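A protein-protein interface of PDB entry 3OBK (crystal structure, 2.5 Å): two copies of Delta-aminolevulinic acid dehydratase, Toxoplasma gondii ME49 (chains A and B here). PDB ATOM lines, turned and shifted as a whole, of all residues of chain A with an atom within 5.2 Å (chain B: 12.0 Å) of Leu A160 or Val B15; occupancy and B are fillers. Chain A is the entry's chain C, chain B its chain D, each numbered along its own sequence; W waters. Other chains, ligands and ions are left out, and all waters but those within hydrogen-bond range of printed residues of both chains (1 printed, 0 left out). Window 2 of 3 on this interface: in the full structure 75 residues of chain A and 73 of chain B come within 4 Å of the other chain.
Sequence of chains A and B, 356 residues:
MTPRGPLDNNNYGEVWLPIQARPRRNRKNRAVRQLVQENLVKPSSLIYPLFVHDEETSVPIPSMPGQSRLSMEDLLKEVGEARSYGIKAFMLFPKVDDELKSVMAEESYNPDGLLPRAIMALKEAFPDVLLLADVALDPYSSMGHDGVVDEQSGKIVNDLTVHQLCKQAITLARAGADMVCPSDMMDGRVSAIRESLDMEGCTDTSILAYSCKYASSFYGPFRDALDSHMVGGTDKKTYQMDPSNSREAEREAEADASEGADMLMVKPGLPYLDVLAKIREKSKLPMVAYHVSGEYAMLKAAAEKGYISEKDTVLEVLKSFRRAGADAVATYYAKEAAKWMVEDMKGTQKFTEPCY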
ATOM      1  N   VAL A 148      13.271  -1.108 -11.133  1.00  0.00           N
ATOM      2  CA  VAL A 148      14.501  -0.841 -10.424  1.00  0.00           C
ATOM      3  C   VAL A 148      14.626   0.653 -10.104  1.00  0.00           C
ATOM      4  O   VAL A 148      14.535   1.511 -10.987  1.00  0.00           O
ATOM      5  CB  VAL A 148      15.721  -1.334 -11.231  1.00  0.00           C
ATOM      6  CG1 VAL A 148      17.014  -1.034 -10.508  1.00  0.00           C
ATOM      7  CG2 VAL A 148      15.619  -2.829 -11.481  1.00  0.00           C
ATOM      8  N   VAL A 157      14.375   3.368 -13.077  1.00  0.00           N
ATOM      9  CA  VAL A 157      15.173   3.391 -14.309  1.00  0.00           C
ATOM     10  C   VAL A 157      14.548   2.418 -15.304  1.00  0.00           C
ATOM     11  O   VAL A 157      14.462   1.214 -15.036  1.00  0.00           O
ATOM     12  CB  VAL A 157      16.679   3.079 -14.051  1.00  0.00           C
ATOM     13  CG1 VAL A 157      16.831   1.959 -13.046  1.00  0.00           C
ATOM     14  CG2 VAL A 157      17.414   2.730 -15.357  1.00  0.00           C
ATOM     15  N   ASN A 158      14.097   2.960 -16.436  1.00  0.00           N
ATOM     16  CA  ASN A 158      13.290   2.236 -17.410  1.00  0.00           C
ATOM     17  C   ASN A 158      13.895   0.968 -18.001  1.00  0.00           C
ATOM     18  O   ASN A 158      13.295  -0.084 -17.936  1.00  0.00           O
ATOM     19  CB  ASN A 158      12.935   3.155 -18.595  1.00  0.00           C
ATOM     20  CG  ASN A 158      11.786   2.606 -19.418  1.00  0.00           C
ATOM     21  OD1 ASN A 158      10.631   2.817 -19.093  1.00  0.00           O
ATOM     22  ND2 ASN A 158      12.097   1.886 -20.465  1.00  0.00           N
ATOM     23  N   ASP A 159      15.061   1.113 -18.614  1.00  0.00           N
ATOM     24  CA  ASP A 159      15.651   0.078 -19.454  1.00  0.00           C
ATOM     25  C   ASP A 159      16.199  -1.070 -18.615  1.00  0.00           C
ATOM     26  O   ASP A 159      16.016  -2.240 -18.919  1.00  0.00           O
ATOM     27  CB  ASP A 159      16.781   0.680 -20.317  1.00  0.00           C
ATOM     28  CG  ASP A 159      16.272   1.704 -21.355  1.00  0.00           C
ATOM     29  OD1 ASP A 159      15.049   2.011 -21.452  1.00  0.00           O
ATOM     30  OD2 ASP A 159      17.143   2.188 -22.114  1.00  0.00           O
ATOM     31  N   LEU A 160      16.854  -0.721 -17.530  1.00  0.00           N
ATOM     32  CA  LEU A 160      17.283  -1.720 -16.571  1.00  0.00           C
ATOM     33  C   LEU A 160      16.073  -2.556 -16.124  1.00  0.00           C
ATOM     34  O   LEU A 160      16.142  -3.788 -16.065  1.00  0.00           O
ATOM     35  CB  LEU A 160      17.961  -1.055 -15.377  1.00  0.00           C
ATOM     36  CG  LEU A 160      19.045  -1.897 -14.734  1.00  0.00           C
ATOM     37  CD1 LEU A 160      20.039  -2.291 -15.817  1.00  0.00           C
ATOM     38  CD2 LEU A 160      19.743  -1.126 -13.617  1.00  0.00           C
ATOM     39  N   THR A 161      14.965  -1.871 -15.843  1.00  0.00           N
ATOM     40  CA  THR A 161      13.720  -2.533 -15.480  1.00  0.00           C
ATOM     41  C   THR A 161      13.223  -3.452 -16.576  1.00  0.00           C
ATOM     42  O   THR A 161      12.875  -4.607 -16.322  1.00  0.00           O
ATOM     43  CB  THR A 161      12.651  -1.505 -15.098  1.00  0.00           C
ATOM     44  OG1 THR A 161      13.167  -0.711 -14.024  1.00  0.00           O
ATOM     45  CG2 THR A 161      11.364  -2.182 -14.656  1.00  0.00           C
ATOM     46  N   VAL A 162      13.236  -2.976 -17.806  1.00  0.00           N
ATOM     47  CA  VAL A 162      12.823  -3.834 -18.931  1.00  0.00           C
ATOM     48  C   VAL A 162      13.691  -5.096 -19.022  1.00  0.00           C
ATOM     49  O   VAL A 162      13.175  -6.198 -19.197  1.00  0.00           O
ATOM     50  CB  VAL A 162      12.815  -3.077 -20.255  1.00  0.00           C
ATOM     51  CG1 VAL A 162      12.651  -4.031 -21.420  1.00  0.00           C
ATOM     52  CG2 VAL A 162      11.704  -2.025 -20.236  1.00  0.00           C
ATOM     53  N   HIS A 163      14.997  -4.933 -18.861  1.00  0.00           N
ATOM     54  CA  HIS A 163      15.909  -6.089 -18.783  1.00  0.00           C
ATOM     55  C   HIS A 163      15.441  -7.110 -17.754  1.00  0.00           C
ATOM     56  O   HIS A 163      15.384  -8.288 -18.054  1.00  0.00           O
ATOM     57  CB  HIS A 163      17.364  -5.668 -18.498  1.00  0.00           C
ATOM     58  CG  HIS A 163      18.369  -6.777 -18.656  1.00  0.00           C
ATOM     59  ND1 HIS A 163      18.877  -7.472 -17.586  1.00  0.00           N
ATOM     60  CD2 HIS A 163      18.961  -7.300 -19.754  1.00  0.00           C
ATOM     61  CE1 HIS A 163      19.725  -8.381 -18.019  1.00  0.00           C
ATOM     62  NE2 HIS A 163      19.803  -8.290 -19.329  1.00  0.00           N
ATOM     63  N   GLN A 164      15.059  -6.666 -16.566  1.00  0.00           N
ATOM     64  CA  GLN A 164      14.583  -7.617 -15.533  1.00  0.00           C
ATOM     65  C   GLN A 164      13.232  -8.242 -15.893  1.00  0.00           C
ATOM     66  O   GLN A 164      13.020  -9.425 -15.680  1.00  0.00           O
ATOM     67  CB  GLN A 164      14.469  -6.934 -14.177  1.00  0.00           C
ATOM     68  CG  GLN A 164      15.754  -6.353 -13.714  1.00  0.00           C
ATOM     69  CD  GLN A 164      16.466  -7.257 -12.787  1.00  0.00           C
ATOM     70  OE1 GLN A 164      17.385  -8.040 -13.189  1.00  0.00           O
ATOM     71  NE2 GLN A 164      16.048  -7.192 -11.502  1.00  0.00           N
ATOM     72  N   GLY B   5      20.115  -9.921 -29.031  1.00  0.00           N
ATOM     73  CA  GLY B   5      18.987  -9.592 -28.111  1.00  0.00           C
ATOM     74  C   GLY B   5      18.546  -8.148 -28.261  1.00  0.00           C
ATOM     75  O   GLY B   5      19.192  -7.379 -28.977  1.00  0.00           O
ATOM     76  N   PRO B   6      17.447  -7.765 -27.575  1.00  0.00           N
ATOM     77  CA  PRO B   6      16.808  -6.441 -27.753  1.00  0.00           C
ATOM     78  C   PRO B   6      17.558  -5.250 -27.160  1.00  0.00           C
ATOM     79  O   PRO B   6      17.498  -4.160 -27.727  1.00  0.00           O
ATOM     80  CB  PRO B   6      15.456  -6.603 -27.053  1.00  0.00           C
ATOM     81  CG  PRO B   6      15.676  -7.701 -26.036  1.00  0.00           C
ATOM     82  CD  PRO B   6      16.728  -8.607 -26.597  1.00  0.00           C
ATOM     83  N   LEU B   7      18.241  -5.452 -26.039  1.00  0.00           N
ATOM     84  CA  LEU B   7      18.957  -4.373 -25.358  1.00  0.00           C
ATOM     85  C   LEU B   7      20.374  -4.199 -25.877  1.00  0.00           C
ATOM     86  O   LEU B   7      20.977  -5.127 -26.383  1.00  0.00           O
ATOM     87  CB  LEU B   7      19.003  -4.638 -23.859  1.00  0.00           C
ATOM     88  CG  LEU B   7      17.631  -4.563 -23.188  1.00  0.00           C
ATOM     89  CD1 LEU B   7      17.587  -5.523 -22.040  1.00  0.00           C
ATOM     90  CD2 LEU B   7      17.340  -3.165 -22.720  1.00  0.00           C
ATOM     91  N   ASP B   8      20.891  -2.988 -25.732  1.00  0.00           N
ATOM     92  CA  ASP B   8      22.236  -2.648 -26.146  1.00  0.00           C
ATOM     93  C   ASP B   8      22.864  -1.887 -24.993  1.00  0.00           C
ATOM     94  O   ASP B   8      22.400  -1.968 -23.862  1.00  0.00           O
ATOM     95  CB  ASP B   8      22.176  -1.783 -27.415  1.00  0.00           C
ATOM     96  CG  ASP B   8      23.471  -1.822 -28.257  1.00  0.00           C
ATOM     97  OD1 ASP B   8      24.588  -2.116 -27.726  1.00  0.00           O
ATOM     98  OD2 ASP B   8      23.334  -1.522 -29.469  1.00  0.00           O
ATOM     99  N   ASN B   9      23.921  -1.149 -25.280  1.00  0.00           N
ATOM    100  CA  ASN B   9      24.610  -0.423 -24.264  1.00  0.00           C
ATOM    101  C   ASN B   9      24.960   0.967 -24.756  1.00  0.00           C
ATOM    102  O   ASN B   9      25.369   1.150 -25.885  1.00  0.00           O
ATOM    103  CB  ASN B   9      25.857  -1.204 -23.839  1.00  0.00           C
ATOM    104  CG  ASN B   9      25.514  -2.543 -23.215  1.00  0.00           C
ATOM    105  OD1 ASN B   9      25.448  -3.554 -23.905  1.00  0.00           O
ATOM    106  ND2 ASN B   9      25.266  -2.550 -21.912  1.00  0.00           N
ATOM    107  N   ASN B  10      24.779   1.955 -23.898  1.00  0.00           N
ATOM    108  CA  ASN B  10      25.131   3.317 -24.236  1.00  0.00           C
ATOM    109  C   ASN B  10      26.652   3.553 -24.141  1.00  0.00           C
ATOM    110  O   ASN B  10      27.413   2.619 -23.912  1.00  0.00           O
ATOM    111  CB  ASN B  10      24.313   4.292 -23.389  1.00  0.00           C
ATOM    112  CG  ASN B  10      24.809   4.413 -21.967  1.00  0.00           C
ATOM    113  OD1 ASN B  10      25.911   4.009 -21.640  1.00  0.00           O
ATOM    114  ND2 ASN B  10      23.993   5.009 -21.116  1.00  0.00           N
ATOM    115  N   ASN B  11      27.075   4.798 -24.330  1.00  0.00           N
ATOM    116  CA  ASN B  11      28.499   5.151 -24.397  1.00  0.00           C
ATOM    117  C   ASN B  11      29.286   5.012 -23.077  1.00  0.00           C
ATOM    118  O   ASN B  11      30.517   5.035 -23.092  1.00  0.00           O
ATOM    119  CB  ASN B  11      28.655   6.577 -24.934  1.00  0.00           C
ATOM    120  CG  ASN B  11      28.208   6.715 -26.380  1.00  0.00           C
ATOM    121  OD1 ASN B  11      28.351   5.788 -27.178  1.00  0.00           O
ATOM    122  ND2 ASN B  11      27.684   7.891 -26.728  1.00  0.00           N
ATOM    123  N   TYR B  12      28.572   4.896 -21.959  1.00  0.00           N
ATOM    124  CA  TYR B  12      29.152   4.541 -20.663  1.00  0.00           C
ATOM    125  C   TYR B  12      28.951   3.038 -20.355  1.00  0.00           C
ATOM    126  O   TYR B  12      29.239   2.588 -19.257  1.00  0.00           O
ATOM    127  CB  TYR B  12      28.542   5.410 -19.541  1.00  0.00           C
ATOM    128  CG  TYR B  12      28.701   6.899 -19.762  1.00  0.00           C
ATOM    129  CD1 TYR B  12      29.698   7.621 -19.122  1.00  0.00           C
ATOM    130  CD2 TYR B  12      27.856   7.585 -20.626  1.00  0.00           C
ATOM    131  CE1 TYR B  12      29.858   9.004 -19.345  1.00  0.00           C
ATOM    132  CE2 TYR B  12      28.000   8.953 -20.855  1.00  0.00           C
ATOM    133  CZ  TYR B  12      29.001   9.663 -20.217  1.00  0.00           C
ATOM    134  OH  TYR B  12      29.128  11.020 -20.471  1.00  0.00           O
ATOM    135  N   GLY B  13      28.452   2.267 -21.321  1.00  0.00           N
ATOM    136  CA  GLY B  13      28.192   0.844 -21.107  1.00  0.00           C
ATOM    137  C   GLY B  13      26.921   0.443 -20.354  1.00  0.00           C
ATOM    138  O   GLY B  13      26.686  -0.739 -20.128  1.00  0.00           O
ATOM    139  N   GLU B  14      26.100   1.419 -19.972  1.00  0.00           N
ATOM    140  CA  GLU B  14      24.857   1.153 -19.253  1.00  0.00           C
ATOM    141  C   GLU B  14      23.839   0.504 -20.184  1.00  0.00           C
ATOM    142  O   GLU B  14      23.828   0.788 -21.386  1.00  0.00           O
ATOM    143  CB  GLU B  14      24.245   2.443 -18.709  1.00  0.00           C
ATOM    144  CG  GLU B  14      25.069   3.168 -17.668  1.00  0.00           C
ATOM    145  CD  GLU B  14      24.594   4.611 -17.453  1.00  0.00           C
ATOM    146  OE1 GLU B  14      24.009   5.201 -18.381  1.00  0.00           O
ATOM    147  OE2 GLU B  14      24.806   5.169 -16.361  1.00  0.00           O
ATOM    148  N   VAL B  15      22.995  -0.346 -19.608  1.00  0.00           N
ATOM    149  CA  VAL B  15      21.940  -1.018 -20.339  1.00  0.00           C
ATOM    150  C   VAL B  15      21.028   0.010 -20.946  1.00  0.00           C
ATOM    151  O   VAL B  15      20.616   0.948 -20.270  1.00  0.00           O
ATOM    152  CB  VAL B  15      21.087  -1.909 -19.428  1.00  0.00           C
ATOM    153  CG1 VAL B  15      19.868  -2.448 -20.183  1.00  0.00           C
ATOM    154  CG2 VAL B  15      21.942  -3.036 -18.840  1.00  0.00           C
ATOM    155  N   TRP B  16      20.718  -0.185 -22.218  1.00  0.00           N
ATOM    156  CA  TRP B  16      20.014   0.803 -23.006  1.00  0.00           C
ATOM    157  C   TRP B  16      19.128   0.111 -24.040  1.00  0.00           C
ATOM    158  O   TRP B  16      19.604  -0.668 -24.857  1.00  0.00           O
ATOM    159  CB  TRP B  16      21.034   1.749 -23.663  1.00  0.00           C
ATOM    160  CG  TRP B  16      20.473   2.632 -24.723  1.00  0.00           C
ATOM    161  CD1 TRP B  16      19.309   3.338 -24.665  1.00  0.00           C
ATOM    162  CD2 TRP B  16      21.038   2.907 -26.009  1.00  0.00           C
ATOM    163  NE1 TRP B  16      19.111   4.029 -25.829  1.00  0.00           N
ATOM    164  CE2 TRP B  16      20.157   3.784 -26.671  1.00  0.00           C
ATOM    165  CE3 TRP B  16      22.204   2.494 -26.669  1.00  0.00           C
ATOM    166  CZ2 TRP B  16      20.405   4.263 -27.951  1.00  0.00           C
ATOM    167  CZ3 TRP B  16      22.454   2.974 -27.943  1.00  0.00           C
ATOM    168  CH2 TRP B  16      21.553   3.843 -28.574  1.00  0.00           C
ATOM    169  N   LEU B  17      17.826   0.378 -23.966  1.00  0.00           N
ATOM    170  CA  LEU B  17      16.850  -0.102 -24.956  1.00  0.00           C
ATOM    171  C   LEU B  17      16.751   1.024 -25.991  1.00  0.00           C
ATOM    172  O   LEU B  17      16.362   2.139 -25.648  1.00  0.00           O
ATOM    173  CB  LEU B  17      15.500  -0.403 -24.286  1.00  0.00           C
ATOM    174  CG  LEU B  17      14.243  -0.864 -25.063  1.00  0.00           C
ATOM    175  CD1 LEU B  17      14.233  -2.332 -25.473  1.00  0.00           C
ATOM    176  CD2 LEU B  17      13.007  -0.606 -24.220  1.00  0.00           C
ATOM    177  N   PRO B  18      17.143   0.762 -27.253  1.00  0.00           N
ATOM    178  CA  PRO B  18      17.189   1.857 -28.253  1.00  0.00           C
ATOM    179  C   PRO B  18      15.854   2.330 -28.815  1.00  0.00           C
ATOM    180  O   PRO B  18      15.727   2.536 -30.020  1.00  0.00           O
ATOM    181  CB  PRO B  18      18.059   1.276 -29.383  1.00  0.00           C
ATOM    182  CG  PRO B  18      18.628   0.030 -28.852  1.00  0.00           C
ATOM    183  CD  PRO B  18      17.762  -0.462 -27.775  1.00  0.00           C
ATOM    184  N   ILE B  19      14.889   2.557 -27.951  1.00  0.00           N
ATOM    185  CA  ILE B  19      13.575   3.001 -28.393  1.00  0.00           C
ATOM    186  C   ILE B  19      13.589   4.535 -28.565  1.00  0.00           C
ATOM    187  O   ILE B  19      14.177   5.239 -27.765  1.00  0.00           O
ATOM    188  CB  ILE B  19      12.479   2.480 -27.404  1.00  0.00           C
ATOM    189  CG1 ILE B  19      11.074   2.769 -27.965  1.00  0.00           C
ATOM    190  CG2 ILE B  19      12.706   3.047 -26.036  1.00  0.00           C
ATOM    191  CD1 ILE B  19       9.921   2.144 -27.240  1.00  0.00           C
ATOM    192  N   ARG B  22       9.529   7.846 -25.945  1.00  0.00           N
ATOM    193  CA  ARG B  22       9.387   7.450 -24.553  1.00  0.00           C
ATOM    194  C   ARG B  22       8.271   8.272 -23.910  1.00  0.00           C
ATOM    195  O   ARG B  22       8.462   9.427 -23.592  1.00  0.00           O
ATOM    196  CB  ARG B  22      10.708   7.651 -23.806  1.00  0.00           C
ATOM    197  CG  ARG B  22      11.803   6.688 -24.248  1.00  0.00           C
ATOM    198  CD  ARG B  22      13.113   6.941 -23.502  1.00  0.00           C
ATOM    199  NE  ARG B  22      14.188   6.033 -23.960  1.00  0.00           N
ATOM    200  CZ  ARG B  22      14.517   4.866 -23.398  1.00  0.00           C
ATOM    201  NH1 ARG B  22      13.870   4.407 -22.335  1.00  0.00           N
ATOM    202  NH2 ARG B  22      15.515   4.155 -23.913  1.00  0.00           N
ATOM    203  N   ARG B  24       7.072   8.061 -20.896  1.00  0.00           N
ATOM    204  CA  ARG B  24       7.423   8.439 -19.537  1.00  0.00           C
ATOM    205  C   ARG B  24       8.105   9.794 -19.443  1.00  0.00           C
ATOM    206  O   ARG B  24       8.102  10.419 -18.365  1.00  0.00           O
ATOM    207  CB  ARG B  24       8.327   7.380 -18.942  1.00  0.00           C
ATOM    208  CG  ARG B  24       7.614   6.037 -18.694  1.00  0.00           C
ATOM    209  CD  ARG B  24       8.562   5.109 -17.945  1.00  0.00           C
ATOM    210  NE  ARG B  24       8.849   5.686 -16.648  1.00  0.00           N
ATOM    211  CZ  ARG B  24       9.868   5.362 -15.867  1.00  0.00           C
ATOM    212  NH1 ARG B  24      10.755   4.438 -16.236  1.00  0.00           N
ATOM    213  NH2 ARG B  24       9.987   5.964 -14.690  1.00  0.00           N
HETATM  214  O   HOH W   1      11.508   5.322 -20.906  1.00  0.00           O
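Of the 9 printed residues of chain A, 4 touch a printed residue of chain B.
Hydrophobic or aromatic side chains of chain A that line the printed part of chain B: Leu A160 and His A163.
Hydrophobic or aromatic side chains of chain B that line the printed part of chain A: Leu B7, Val B15, Trp B16 and Leu B17.
Among the printed residues, 8 pairs touch across the chains.
Among the printed residues, Asp or Glu carboxylates within 4 Å of a Lys or Arg side-chain nitrogen of the other chain: Asp A159 with Arg B22 (2.8 Å).
The side-chain carboxylate (OD1) of Asp A159 lies within salt-bridge range of the guanidinium group (NH1) of Arg B22 (2.8 Å).
The guanidinium group of Arg B24 sits at hydrogen-bond distance from the side-chain amide oxygen of Asn A158 (3.3 Å).
The side-chain carboxylate of Asp A159 is in hydrogen-bond range of the backbone NH of Leu B17, at 2.7 Å.
No residue of chain B comes within 4 Å of Val A157.
Asp A159 touches four residues of chain B.
Of chain B, only Val B15 (3.6 Å) comes within 4 Å of Leu A160.
No residue of chain B comes within 4 Å of Val A162.
Of the printed residues of chain B, His A163 touches Leu B7.
No residue of chain B comes within 4 Å of Gln A164.
Of the printed residues of chain A, Leu B7 touches His A163.
Asn B11 touches none of the printed residues of chain A.
Val B15 touches two residues of chain A.
Of the printed residues of chain A, Trp B16 touches Asp A159.
Printed residues of chain A within 4 Å of Leu B17: Asp A159.
Printed residues of chain A within 4 Å of Arg B22: Asn A158 and Asp A159.
The nearest residue of chain B that does not touch Leu A160 is Leu B7 (5.8 Å).
The nearest residue of chain A that does not touch Val B15 is His A163 (4.4 Å).
The nearest printed residue of chain A that does not touch Arg B24 is Val A157 (4.4 Å).
No position is printed for both chains.
Of the 8 pairs that touch across the chains among the printed residues, none has its exchanged pair printed and touching as well.
Arg B22 touches Asn A158 (NH1 to ND2, 3.6 Å).
Val B15 touches Asp A159 (O to CB, 3.8 Å).
OD2 of Asp A159 touches CA of Trp B16, 3.3 Å away.
CD1 of Leu A160 touches CG2 of Val B15, 3.6 Å away.
His A163 touches Leu B7.
The backbone carbonyl oxygen (O) of Trp B16 lies within hydrogen-bond range of the backbone NH (N) of Asp B8 (2.8 Å).
The guanidinium group of Arg B22 is in hydrogen-bond range of the backbone carbonyl oxygen of Leu B17 (2.8 Å).
The side-chain amide nitrogen (ND2) of Asn A158 sits at hydrogen-bond distance from the side-chain carboxylate (OD1) of Asp A159, 3.1 Å away.
Water W1 lies within hydrogen-bond range of the guanidinium group of Arg B22 and the side-chain amide oxygen of Asn A158.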
